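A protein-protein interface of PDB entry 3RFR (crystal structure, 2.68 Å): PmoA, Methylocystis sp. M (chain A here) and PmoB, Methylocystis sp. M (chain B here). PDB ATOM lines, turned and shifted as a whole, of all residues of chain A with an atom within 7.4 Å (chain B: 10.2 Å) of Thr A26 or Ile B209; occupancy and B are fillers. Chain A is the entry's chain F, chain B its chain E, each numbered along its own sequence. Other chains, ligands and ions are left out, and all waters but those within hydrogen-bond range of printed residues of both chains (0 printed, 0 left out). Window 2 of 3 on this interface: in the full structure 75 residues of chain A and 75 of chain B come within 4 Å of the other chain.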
ATOM      1  N   ALA A  20     -22.113  21.742  -7.243  1.00  0.00           N
ATOM      2  CA  ALA A  20     -21.619  21.896  -8.599  1.00  0.00           C
ATOM      3  C   ALA A  20     -20.604  20.806  -8.894  1.00  0.00           C
ATOM      4  O   ALA A  20     -20.610  20.233  -9.980  1.00  0.00           O
ATOM      5  CB  ALA A  20     -21.003  23.289  -8.788  1.00  0.00           C
ATOM      6  N   GLY A  21     -19.750  20.527  -7.913  1.00  0.00           N
ATOM      7  CA  GLY A  21     -18.680  19.558  -8.060  1.00  0.00           C
ATOM      8  C   GLY A  21     -19.257  18.177  -8.230  1.00  0.00           C
ATOM      9  O   GLY A  21     -18.694  17.337  -8.928  1.00  0.00           O
ATOM     10  N   CYS A  22     -20.402  17.947  -7.598  1.00  0.00           N
ATOM     11  CA  CYS A  22     -21.100  16.668  -7.714  1.00  0.00           C
ATOM     12  C   CYS A  22     -21.776  16.506  -9.062  1.00  0.00           C
ATOM     13  O   CYS A  22     -21.702  15.453  -9.667  1.00  0.00           O
ATOM     14  CB  CYS A  22     -22.142  16.519  -6.607  1.00  0.00           C
ATOM     15  SG  CYS A  22     -22.577  14.804  -6.265  1.00  0.00           S
ATOM     16  N   VAL A  23     -22.447  17.551  -9.521  1.00  0.00           N
ATOM     17  CA  VAL A  23     -23.208  17.479 -10.752  1.00  0.00           C
ATOM     18  C   VAL A  23     -22.278  17.177 -11.925  1.00  0.00           C
ATOM     19  O   VAL A  23     -22.544  16.236 -12.689  1.00  0.00           O
ATOM     20  CB  VAL A  23     -24.069  18.758 -10.973  1.00  0.00           C
ATOM     21  CG1 VAL A  23     -24.538  18.868 -12.394  1.00  0.00           C
ATOM     22  CG2 VAL A  23     -25.277  18.746 -10.047  1.00  0.00           C
ATOM     23  N   ALA A  24     -21.188  17.935 -12.036  1.00  0.00           N
ATOM     24  CA  ALA A  24     -20.195  17.765 -13.104  1.00  0.00           C
ATOM     25  C   ALA A  24     -19.510  16.391 -13.099  1.00  0.00           C
ATOM     26  O   ALA A  24     -19.242  15.836 -14.162  1.00  0.00           O
ATOM     27  CB  ALA A  24     -19.129  18.907 -13.075  1.00  0.00           C
ATOM     28  N   THR A  25     -19.211  15.835 -11.925  1.00  0.00           N
ATOM     29  CA  THR A  25     -18.494  14.553 -11.912  1.00  0.00           C
ATOM     30  C   THR A  25     -19.386  13.332 -11.945  1.00  0.00           C
ATOM     31  O   THR A  25     -18.932  12.272 -12.312  1.00  0.00           O
ATOM     32  CB  THR A  25     -17.387  14.419 -10.809  1.00  0.00           C
ATOM     33  OG1 THR A  25     -17.974  14.093  -9.554  1.00  0.00           O
ATOM     34  CG2 THR A  25     -16.510  15.683 -10.711  1.00  0.00           C
ATOM     35  N   THR A  26     -20.649  13.478 -11.573  1.00  0.00           N
ATOM     36  CA  THR A  26     -21.621  12.429 -11.839  1.00  0.00           C
ATOM     37  C   THR A  26     -21.933  12.433 -13.325  1.00  0.00           C
ATOM     38  O   THR A  26     -22.203  11.388 -13.901  1.00  0.00           O
ATOM     39  CB  THR A  26     -22.920  12.589 -11.017  1.00  0.00           C
ATOM     40  OG1 THR A  26     -22.648  12.329  -9.641  1.00  0.00           O
ATOM     41  CG2 THR A  26     -24.003  11.599 -11.491  1.00  0.00           C
ATOM     42  N   ASP A  27     -21.888  13.621 -13.929  1.00  0.00           N
ATOM     43  CA  ASP A  27     -22.153  13.772 -15.347  1.00  0.00           C
ATOM     44  C   ASP A  27     -21.151  12.970 -16.186  1.00  0.00           C
ATOM     45  O   ASP A  27     -21.547  12.246 -17.116  1.00  0.00           O
ATOM     46  CB  ASP A  27     -22.203  15.258 -15.750  1.00  0.00           C
ATOM     47  CG  ASP A  27     -23.646  15.816 -15.819  1.00  0.00           C
ATOM     48  OD1 ASP A  27     -24.533  15.330 -15.100  1.00  0.00           O
ATOM     49  OD2 ASP A  27     -23.905  16.745 -16.610  1.00  0.00           O
ATOM     50  N   TRP A  28     -19.865  13.070 -15.843  1.00  0.00           N
ATOM     51  CA  TRP A  28     -18.816  12.325 -16.558  1.00  0.00           C
ATOM     52  C   TRP A  28     -19.092  10.847 -16.427  1.00  0.00           C
ATOM     53  O   TRP A  28     -19.195  10.142 -17.433  1.00  0.00           O
ATOM     54  CB  TRP A  28     -17.401  12.646 -16.045  1.00  0.00           C
ATOM     55  CG  TRP A  28     -16.780  13.859 -16.685  1.00  0.00           C
ATOM     56  CD1 TRP A  28     -16.539  15.086 -16.095  1.00  0.00           C
ATOM     57  CD2 TRP A  28     -16.336  13.979 -18.050  1.00  0.00           C
ATOM     58  NE1 TRP A  28     -15.962  15.949 -17.007  1.00  0.00           N
ATOM     59  CE2 TRP A  28     -15.815  15.297 -18.209  1.00  0.00           C
ATOM     60  CE3 TRP A  28     -16.283  13.089 -19.145  1.00  0.00           C
ATOM     61  CZ2 TRP A  28     -15.282  15.752 -19.432  1.00  0.00           C
ATOM     62  CZ3 TRP A  28     -15.747  13.540 -20.354  1.00  0.00           C
ATOM     63  CH2 TRP A  28     -15.263  14.863 -20.488  1.00  0.00           C
ATOM     64  N   MET A  29     -19.249  10.391 -15.189  1.00  0.00           N
ATOM     65  CA  MET A  29     -19.392   8.975 -14.910  1.00  0.00           C
ATOM     66  C   MET A  29     -20.549   8.366 -15.705  1.00  0.00           C
ATOM     67  O   MET A  29     -20.435   7.244 -16.204  1.00  0.00           O
ATOM     68  CB  MET A  29     -19.644   8.763 -13.429  1.00  0.00           C
ATOM     69  CG  MET A  29     -18.484   9.027 -12.504  1.00  0.00           C
ATOM     70  SD  MET A  29     -19.079   9.047 -10.805  1.00  0.00           S
ATOM     71  CE  MET A  29     -19.238   7.317 -10.434  1.00  0.00           C
ATOM     72  N   LEU A  30     -21.663   9.097 -15.808  1.00  0.00           N
ATOM     73  CA  LEU A  30     -22.856   8.610 -16.501  1.00  0.00           C
ATOM     74  C   LEU A  30     -22.611   8.499 -17.998  1.00  0.00           C
ATOM     75  O   LEU A  30     -23.011   7.490 -18.610  1.00  0.00           O
ATOM     76  CB  LEU A  30     -24.074   9.488 -16.256  1.00  0.00           C
ATOM     77  CG  LEU A  30     -24.784   9.504 -14.907  1.00  0.00           C
ATOM     78  CD1 LEU A  30     -25.898  10.527 -14.966  1.00  0.00           C
ATOM     79  CD2 LEU A  30     -25.340   8.151 -14.511  1.00  0.00           C
ATOM     80  N   LEU A  31     -21.963   9.518 -18.574  1.00  0.00           N
ATOM     81  CA  LEU A  31     -21.527   9.487 -19.973  1.00  0.00           C
ATOM     82  C   LEU A  31     -20.534   8.339 -20.260  1.00  0.00           C
ATOM     83  O   LEU A  31     -20.598   7.704 -21.306  1.00  0.00           O
ATOM     84  CB  LEU A  31     -20.914  10.836 -20.375  1.00  0.00           C
ATOM     85  CG  LEU A  31     -20.592  11.128 -21.842  1.00  0.00           C
ATOM     86  CD1 LEU A  31     -21.815  11.550 -22.630  1.00  0.00           C
ATOM     87  CD2 LEU A  31     -19.533  12.215 -21.875  1.00  0.00           C
ATOM     88  N   VAL A  32     -19.635   8.078 -19.319  1.00  0.00           N
ATOM     89  CA  VAL A  32     -18.590   7.069 -19.496  1.00  0.00           C
ATOM     90  C   VAL A  32     -19.163   5.694 -19.304  1.00  0.00           C
ATOM     91  O   VAL A  32     -18.778   4.786 -20.010  1.00  0.00           O
ATOM     92  CB  VAL A  32     -17.356   7.306 -18.534  1.00  0.00           C
ATOM     93  CG1 VAL A  32     -16.339   6.179 -18.600  1.00  0.00           C
ATOM     94  CG2 VAL A  32     -16.659   8.574 -18.905  1.00  0.00           C
ATOM     95  N   LEU A  33     -20.082   5.540 -18.352  1.00  0.00           N
ATOM     96  CA  LEU A  33     -20.780   4.258 -18.178  1.00  0.00           C
ATOM     97  C   LEU A  33     -21.698   3.995 -19.337  1.00  0.00           C
ATOM     98  O   LEU A  33     -21.792   2.868 -19.753  1.00  0.00           O
ATOM     99  CB  LEU A  33     -21.568   4.165 -16.854  1.00  0.00           C
ATOM    100  CG  LEU A  33     -23.042   4.606 -16.715  1.00  0.00           C
ATOM    101  CD1 LEU A  33     -23.996   3.481 -17.042  1.00  0.00           C
ATOM    102  CD2 LEU A  33     -23.314   5.076 -15.314  1.00  0.00           C
ATOM    103  N   PHE A  88     -33.648  13.740 -22.313  1.00  0.00           N
ATOM    104  CA  PHE A  88     -32.690  14.881 -22.047  1.00  0.00           C
ATOM    105  C   PHE A  88     -32.627  15.950 -23.120  1.00  0.00           C
ATOM    106  O   PHE A  88     -31.909  16.928 -22.966  1.00  0.00           O
ATOM    107  CB  PHE A  88     -31.217  14.477 -21.841  1.00  0.00           C
ATOM    108  CG  PHE A  88     -30.986  13.333 -20.918  1.00  0.00           C
ATOM    109  CD1 PHE A  88     -30.266  13.535 -19.735  1.00  0.00           C
ATOM    110  CD2 PHE A  88     -31.383  12.014 -21.281  1.00  0.00           C
ATOM    111  CE1 PHE A  88     -29.985  12.473 -18.898  1.00  0.00           C
ATOM    112  CE2 PHE A  88     -31.126  10.934 -20.444  1.00  0.00           C
ATOM    113  CZ  PHE A  88     -30.442  11.148 -19.246  1.00  0.00           C
ATOM    114  N   LEU A  90     -30.917  15.650 -25.659  1.00  0.00           N
ATOM    115  CA  LEU A  90     -29.570  15.666 -26.226  1.00  0.00           C
ATOM    116  C   LEU A  90     -29.584  15.026 -27.644  1.00  0.00           C
ATOM    117  O   LEU A  90     -30.042  13.881 -27.849  1.00  0.00           O
ATOM    118  CB  LEU A  90     -28.510  15.067 -25.284  1.00  0.00           C
ATOM    119  CG  LEU A  90     -28.341  15.740 -23.909  1.00  0.00           C
ATOM    120  CD1 LEU A  90     -27.607  14.816 -22.964  1.00  0.00           C
ATOM    121  CD2 LEU A  90     -27.635  17.102 -23.941  1.00  0.00           C
ATOM    122  N   TRP B 202     -22.363  19.066 -27.154  1.00  0.00           N
ATOM    123  CA  TRP B 202     -23.605  19.025 -26.415  1.00  0.00           C
ATOM    124  C   TRP B 202     -23.451  18.688 -24.937  1.00  0.00           C
ATOM    125  O   TRP B 202     -24.050  19.348 -24.095  1.00  0.00           O
ATOM    126  CB  TRP B 202     -24.585  18.114 -27.114  1.00  0.00           C
ATOM    127  CG  TRP B 202     -24.771  18.562 -28.492  1.00  0.00           C
ATOM    128  CD1 TRP B 202     -24.306  17.966 -29.604  1.00  0.00           C
ATOM    129  CD2 TRP B 202     -25.447  19.748 -28.922  1.00  0.00           C
ATOM    130  NE1 TRP B 202     -24.665  18.682 -30.719  1.00  0.00           N
ATOM    131  CE2 TRP B 202     -25.369  19.788 -30.324  1.00  0.00           C
ATOM    132  CE3 TRP B 202     -26.114  20.775 -28.260  1.00  0.00           C
ATOM    133  CZ2 TRP B 202     -25.935  20.813 -31.077  1.00  0.00           C
ATOM    134  CZ3 TRP B 202     -26.663  21.784 -29.010  1.00  0.00           C
ATOM    135  CH2 TRP B 202     -26.574  21.793 -30.405  1.00  0.00           C
ATOM    136  N   PHE B 203     -22.635  17.687 -24.615  1.00  0.00           N
ATOM    137  CA  PHE B 203     -22.418  17.296 -23.232  1.00  0.00           C
ATOM    138  C   PHE B 203     -22.057  18.524 -22.420  1.00  0.00           C
ATOM    139  O   PHE B 203     -22.727  18.841 -21.438  1.00  0.00           O
ATOM    140  CB  PHE B 203     -21.342  16.219 -23.147  1.00  0.00           C
ATOM    141  CG  PHE B 203     -20.922  15.854 -21.741  1.00  0.00           C
ATOM    142  CD1 PHE B 203     -21.777  15.155 -20.885  1.00  0.00           C
ATOM    143  CD2 PHE B 203     -19.646  16.167 -21.292  1.00  0.00           C
ATOM    144  CE1 PHE B 203     -21.364  14.797 -19.595  1.00  0.00           C
ATOM    145  CE2 PHE B 203     -19.220  15.813 -20.016  1.00  0.00           C
ATOM    146  CZ  PHE B 203     -20.081  15.131 -19.161  1.00  0.00           C
ATOM    147  N   ILE B 204     -21.042  19.252 -22.871  1.00  0.00           N
ATOM    148  CA  ILE B 204     -20.543  20.396 -22.125  1.00  0.00           C
ATOM    149  C   ILE B 204     -21.451  21.638 -22.199  1.00  0.00           C
ATOM    150  O   ILE B 204     -21.690  22.267 -21.186  1.00  0.00           O
ATOM    151  CB  ILE B 204     -19.077  20.676 -22.490  1.00  0.00           C
ATOM    152  CG1 ILE B 204     -18.336  21.243 -21.279  1.00  0.00           C
ATOM    153  CG2 ILE B 204     -18.967  21.532 -23.755  1.00  0.00           C
ATOM    154  CD1 ILE B 204     -16.807  21.196 -21.393  1.00  0.00           C
ATOM    155  N   LYS B 206     -24.448  22.666 -21.694  1.00  0.00           N
ATOM    156  CA  LYS B 206     -25.727  22.340 -21.052  1.00  0.00           C
ATOM    157  C   LYS B 206     -25.922  20.823 -21.053  1.00  0.00           C
ATOM    158  O   LYS B 206     -26.327  20.268 -22.075  1.00  0.00           O
ATOM    159  CB  LYS B 206     -26.901  23.115 -21.710  1.00  0.00           C
ATOM    160  CG  LYS B 206     -26.914  24.672 -21.434  1.00  0.00           C
ATOM    161  CD  LYS B 206     -27.493  25.020 -20.052  1.00  0.00           C
ATOM    162  CE  LYS B 206     -26.764  26.199 -19.367  1.00  0.00           C
ATOM    163  NZ  LYS B 206     -27.306  27.549 -19.702  1.00  0.00           N
ATOM    164  N   GLY B 207     -25.676  20.219 -19.873  1.00  0.00           N
ATOM    165  CA  GLY B 207     -25.159  18.847 -19.689  1.00  0.00           C
ATOM    166  C   GLY B 207     -26.116  17.680 -19.491  1.00  0.00           C
ATOM    167  O   GLY B 207     -27.202  17.660 -20.085  1.00  0.00           O
ATOM    168  N   ILE B 208     -25.724  16.688 -18.681  1.00  0.00           N
ATOM    169  CA  ILE B 208     -26.597  15.503 -18.458  1.00  0.00           C
ATOM    170  C   ILE B 208     -27.647  15.698 -17.367  1.00  0.00           C
ATOM    171  O   ILE B 208     -28.806  15.868 -17.699  1.00  0.00           O
ATOM    172  CB  ILE B 208     -25.823  14.184 -18.268  1.00  0.00           C
ATOM    173  CG1 ILE B 208     -25.240  13.726 -19.602  1.00  0.00           C
ATOM    174  CG2 ILE B 208     -26.742  13.109 -17.763  1.00  0.00           C
ATOM    175  CD1 ILE B 208     -24.195  12.663 -19.475  1.00  0.00           C
ATOM    176  N   ILE B 209     -27.251  15.678 -16.090  1.00  0.00           N
ATOM    177  CA  ILE B 209     -28.162  15.998 -14.976  1.00  0.00           C
ATOM    178  C   ILE B 209     -28.928  17.342 -15.133  1.00  0.00           C
ATOM    179  O   ILE B 209     -30.142  17.390 -14.883  1.00  0.00           O
ATOM    180  CB  ILE B 209     -27.445  15.971 -13.587  1.00  0.00           C
ATOM    181  CG1 ILE B 209     -26.949  14.562 -13.237  1.00  0.00           C
ATOM    182  CG2 ILE B 209     -28.375  16.486 -12.487  1.00  0.00           C
ATOM    183  CD1 ILE B 209     -26.097  14.480 -11.978  1.00  0.00           C
ATOM    184  N   ALA B 210     -28.233  18.423 -15.529  1.00  0.00           N
ATOM    185  CA  ALA B 210     -28.889  19.724 -15.718  1.00  0.00           C
ATOM    186  C   ALA B 210     -30.022  19.639 -16.764  1.00  0.00           C
ATOM    187  O   ALA B 210     -31.024  20.349 -16.662  1.00  0.00           O
ATOM    188  CB  ALA B 210     -27.883  20.818 -16.044  1.00  0.00           C
ATOM    189  N   SER B 211     -29.869  18.733 -17.733  1.00  0.00           N
ATOM    190  CA  SER B 211     -30.862  18.484 -18.788  1.00  0.00           C
ATOM    191  C   SER B 211     -31.954  17.515 -18.377  1.00  0.00           C
ATOM    192  O   SER B 211     -33.095  17.630 -18.826  1.00  0.00           O
ATOM    193  CB  SER B 211     -30.187  17.926 -20.042  1.00  0.00           C
ATOM    194  OG  SER B 211     -29.616  18.959 -20.800  1.00  0.00           O
ATOM    195  N   TYR B 212     -31.588  16.522 -17.577  1.00  0.00           N
ATOM    196  CA  TYR B 212     -32.572  15.586 -17.111  1.00  0.00           C
ATOM    197  C   TYR B 212     -33.575  16.380 -16.315  1.00  0.00           C
ATOM    198  O   TYR B 212     -34.780  16.303 -16.580  1.00  0.00           O
ATOM    199  CB  TYR B 212     -31.976  14.497 -16.223  1.00  0.00           C
ATOM    200  CG  TYR B 212     -33.066  13.686 -15.559  1.00  0.00           C
ATOM    201  CD1 TYR B 212     -33.818  12.776 -16.295  1.00  0.00           C
ATOM    202  CD2 TYR B 212     -33.377  13.871 -14.211  1.00  0.00           C
ATOM    203  CE1 TYR B 212     -34.838  12.051 -15.702  1.00  0.00           C
ATOM    204  CE2 TYR B 212     -34.399  13.143 -13.604  1.00  0.00           C
ATOM    205  CZ  TYR B 212     -35.123  12.233 -14.357  1.00  0.00           C
ATOM    206  OH  TYR B 212     -36.126  11.506 -13.777  1.00  0.00           O
ATOM    207  N   VAL B 213     -33.056  17.147 -15.356  1.00  0.00           N
ATOM    208  CA  VAL B 213     -33.861  17.978 -14.504  1.00  0.00           C
ATOM    209  C   VAL B 213     -34.748  18.868 -15.371  1.00  0.00           C
ATOM    210  O   VAL B 213     -35.942  18.876 -15.175  1.00  0.00           O
ATOM    211  CB  VAL B 213     -33.009  18.765 -13.456  1.00  0.00           C
ATOM    212  CG1 VAL B 213     -33.830  19.871 -12.812  1.00  0.00           C
ATOM    213  CG2 VAL B 213     -32.458  17.840 -12.367  1.00  0.00           C
ATOM    214  N   ARG B 214     -34.199  19.556 -16.366  1.00  0.00           N
ATOM    215  CA  ARG B 214     -35.012  20.492 -17.158  1.00  0.00           C
ATOM    216  C   ARG B 214     -36.206  19.879 -17.858  1.00  0.00           C
ATOM    217  O   ARG B 214     -37.306  20.382 -17.765  1.00  0.00           O
ATOM    218  CB  ARG B 214     -34.175  21.235 -18.171  1.00  0.00           C
ATOM    219  CG  ARG B 214     -33.469  22.411 -17.584  1.00  0.00           C
ATOM    220  CD  ARG B 214     -32.737  23.181 -18.642  1.00  0.00           C
ATOM    221  NE  ARG B 214     -31.598  23.875 -18.056  1.00  0.00           N
ATOM    222  CZ  ARG B 214     -30.945  24.872 -18.636  1.00  0.00           C
ATOM    223  NH1 ARG B 214     -31.317  25.302 -19.825  1.00  0.00           N
ATOM    224  NH2 ARG B 214     -29.928  25.444 -18.015  1.00  0.00           N
ATOM    225  N   VAL B 215     -35.975  18.793 -18.571  1.00  0.00           N
ATOM    226  CA  VAL B 215     -37.022  18.037 -19.226  1.00  0.00           C
ATOM    227  C   VAL B 215     -38.030  17.514 -18.202  1.00  0.00           C
ATOM    228  O   VAL B 215     -39.236  17.552 -18.437  1.00  0.00           O
ATOM    229  CB  VAL B 215     -36.389  16.867 -20.036  1.00  0.00           C
ATOM    230  CG1 VAL B 215     -37.422  15.805 -20.433  1.00  0.00           C
ATOM    231  CG2 VAL B 215     -35.661  17.404 -21.257  1.00  0.00           C
ATOM    232  N   ALA B 216     -37.526  17.040 -17.068  1.00  0.00           N
ATOM    233  CA  ALA B 216     -38.357  16.372 -16.091  1.00  0.00           C
ATOM    234  C   ALA B 216     -39.261  17.371 -15.414  1.00  0.00           C
ATOM    235  O   ALA B 216     -40.423  17.060 -15.095  1.00  0.00           O
ATOM    236  CB  ALA B 216     -37.508  15.673 -15.075  1.00  0.00           C
ATOM    237  N   GLU B 217     -38.706  18.567 -15.187  1.00  0.00           N
ATOM    238  CA  GLU B 217     -39.432  19.701 -14.619  1.00  0.00           C
ATOM    239  C   GLU B 217     -40.358  20.242 -15.686  1.00  0.00           C
ATOM    240  O   GLU B 217     -41.149  19.492 -16.269  1.00  0.00           O
ATOM    241  CB  GLU B 217     -38.485  20.802 -14.151  1.00  0.00           C
ATOM    242  CG  GLU B 217     -37.610  20.424 -12.981  1.00  0.00           C
ATOM    243  CD  GLU B 217     -38.201  20.793 -11.649  1.00  0.00           C
ATOM    244  OE1 GLU B 217     -39.068  21.687 -11.611  1.00  0.00           O
ATOM    245  OE2 GLU B 217     -37.788  20.199 -10.634  1.00  0.00           O
ATOM    246  N   VAL B 223     -33.380  23.725 -23.037  1.00  0.00           N
ATOM    247  CA  VAL B 223     -32.299  22.818 -23.441  1.00  0.00           C
ATOM    248  C   VAL B 223     -31.981  23.046 -24.904  1.00  0.00           C
ATOM    249  O   VAL B 223     -30.849  23.332 -25.269  1.00  0.00           O
ATOM    250  CB  VAL B 223     -32.658  21.324 -23.240  1.00  0.00           C
ATOM    251  CG1 VAL B 223     -31.453  20.445 -23.552  1.00  0.00           C
ATOM    252  CG2 VAL B 223     -33.136  21.057 -21.833  1.00  0.00           C
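Of chain B, only Ile B209 (3.6 Å) comes within 4 Å of Thr A26. Of the printed residues of chain A, Ile B209 touches Thr A26 (3.6 Å) and Asp A27 (2.9 Å). No residue of chain B comes within 4 Å of Cys A22. No residue of chain B comes within 4 Å of Ala A24. No residue of chain B comes within 4 Å of Thr A25. Asp A27 touches just these residues of chain B: Phe B203, Gly B207, Ile B208 and Ile B209. No residue of chain B comes within 4 Å of Met A29. Printed residues of chain A within 4 Å of Ile B208: Asp A27, Leu A30, Leu A31 and Phe A88. Of the printed residues of chain A, Phe B203 touches Asp A27, Trp A28 and Leu A31. Printed residues of chain B within 4 Å of Trp A28: Phe B203 (3.9 Å). Of the printed residues of chain B, Leu A90 touches Lys B206 and Gly B207. Of the printed residues of chain A, Lys B206 touches Leu A90 (3.9 Å).
Among the printed residues, merely in contact across the chains: Phe A88 with Ile B208, Phe A88 with Ser B211, Asp A27 with Phe B203, Phe A88 with Val B223, Thr A26 with Ile B209, Asp A27 with Gly B207, Leu A31 with Phe B203, Phe A88 with Val B215, Leu A31 with Ile B208, Trp A28 with Phe B203, Leu A30 with Ile B208, Phe A88 with Tyr B212, Leu A90 with Lys B206 and Leu A90 with Gly B207.
The backbone NH (N) of Ile B208 sits at hydrogen-bond distance from the side-chain carboxylate (OD2) of Asp A27. The backbone NH of Ile B209 sits at hydrogen-bond distance from the side-chain carboxylate of Asp A27.
The backbone carbonyl oxygen (O) of Gly B207 sits at hydrogen-bond distance from the side-chain hydroxyl (OG) of Ser B211 (2.8 Å). The backbone carbonyl oxygen of Cys A22 lies within hydrogen-bond range of the side-chain hydroxyl of Thr A26 (3.3 Å).
Hydrophobic or aromatic side chains of chain B that line the printed part of chain A: Phe B203, Ile B208, Ile B209, Tyr B212, Val B215 and Val B223. Of the 16 printed residues of chain A, 7 touch a printed residue of chain B.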
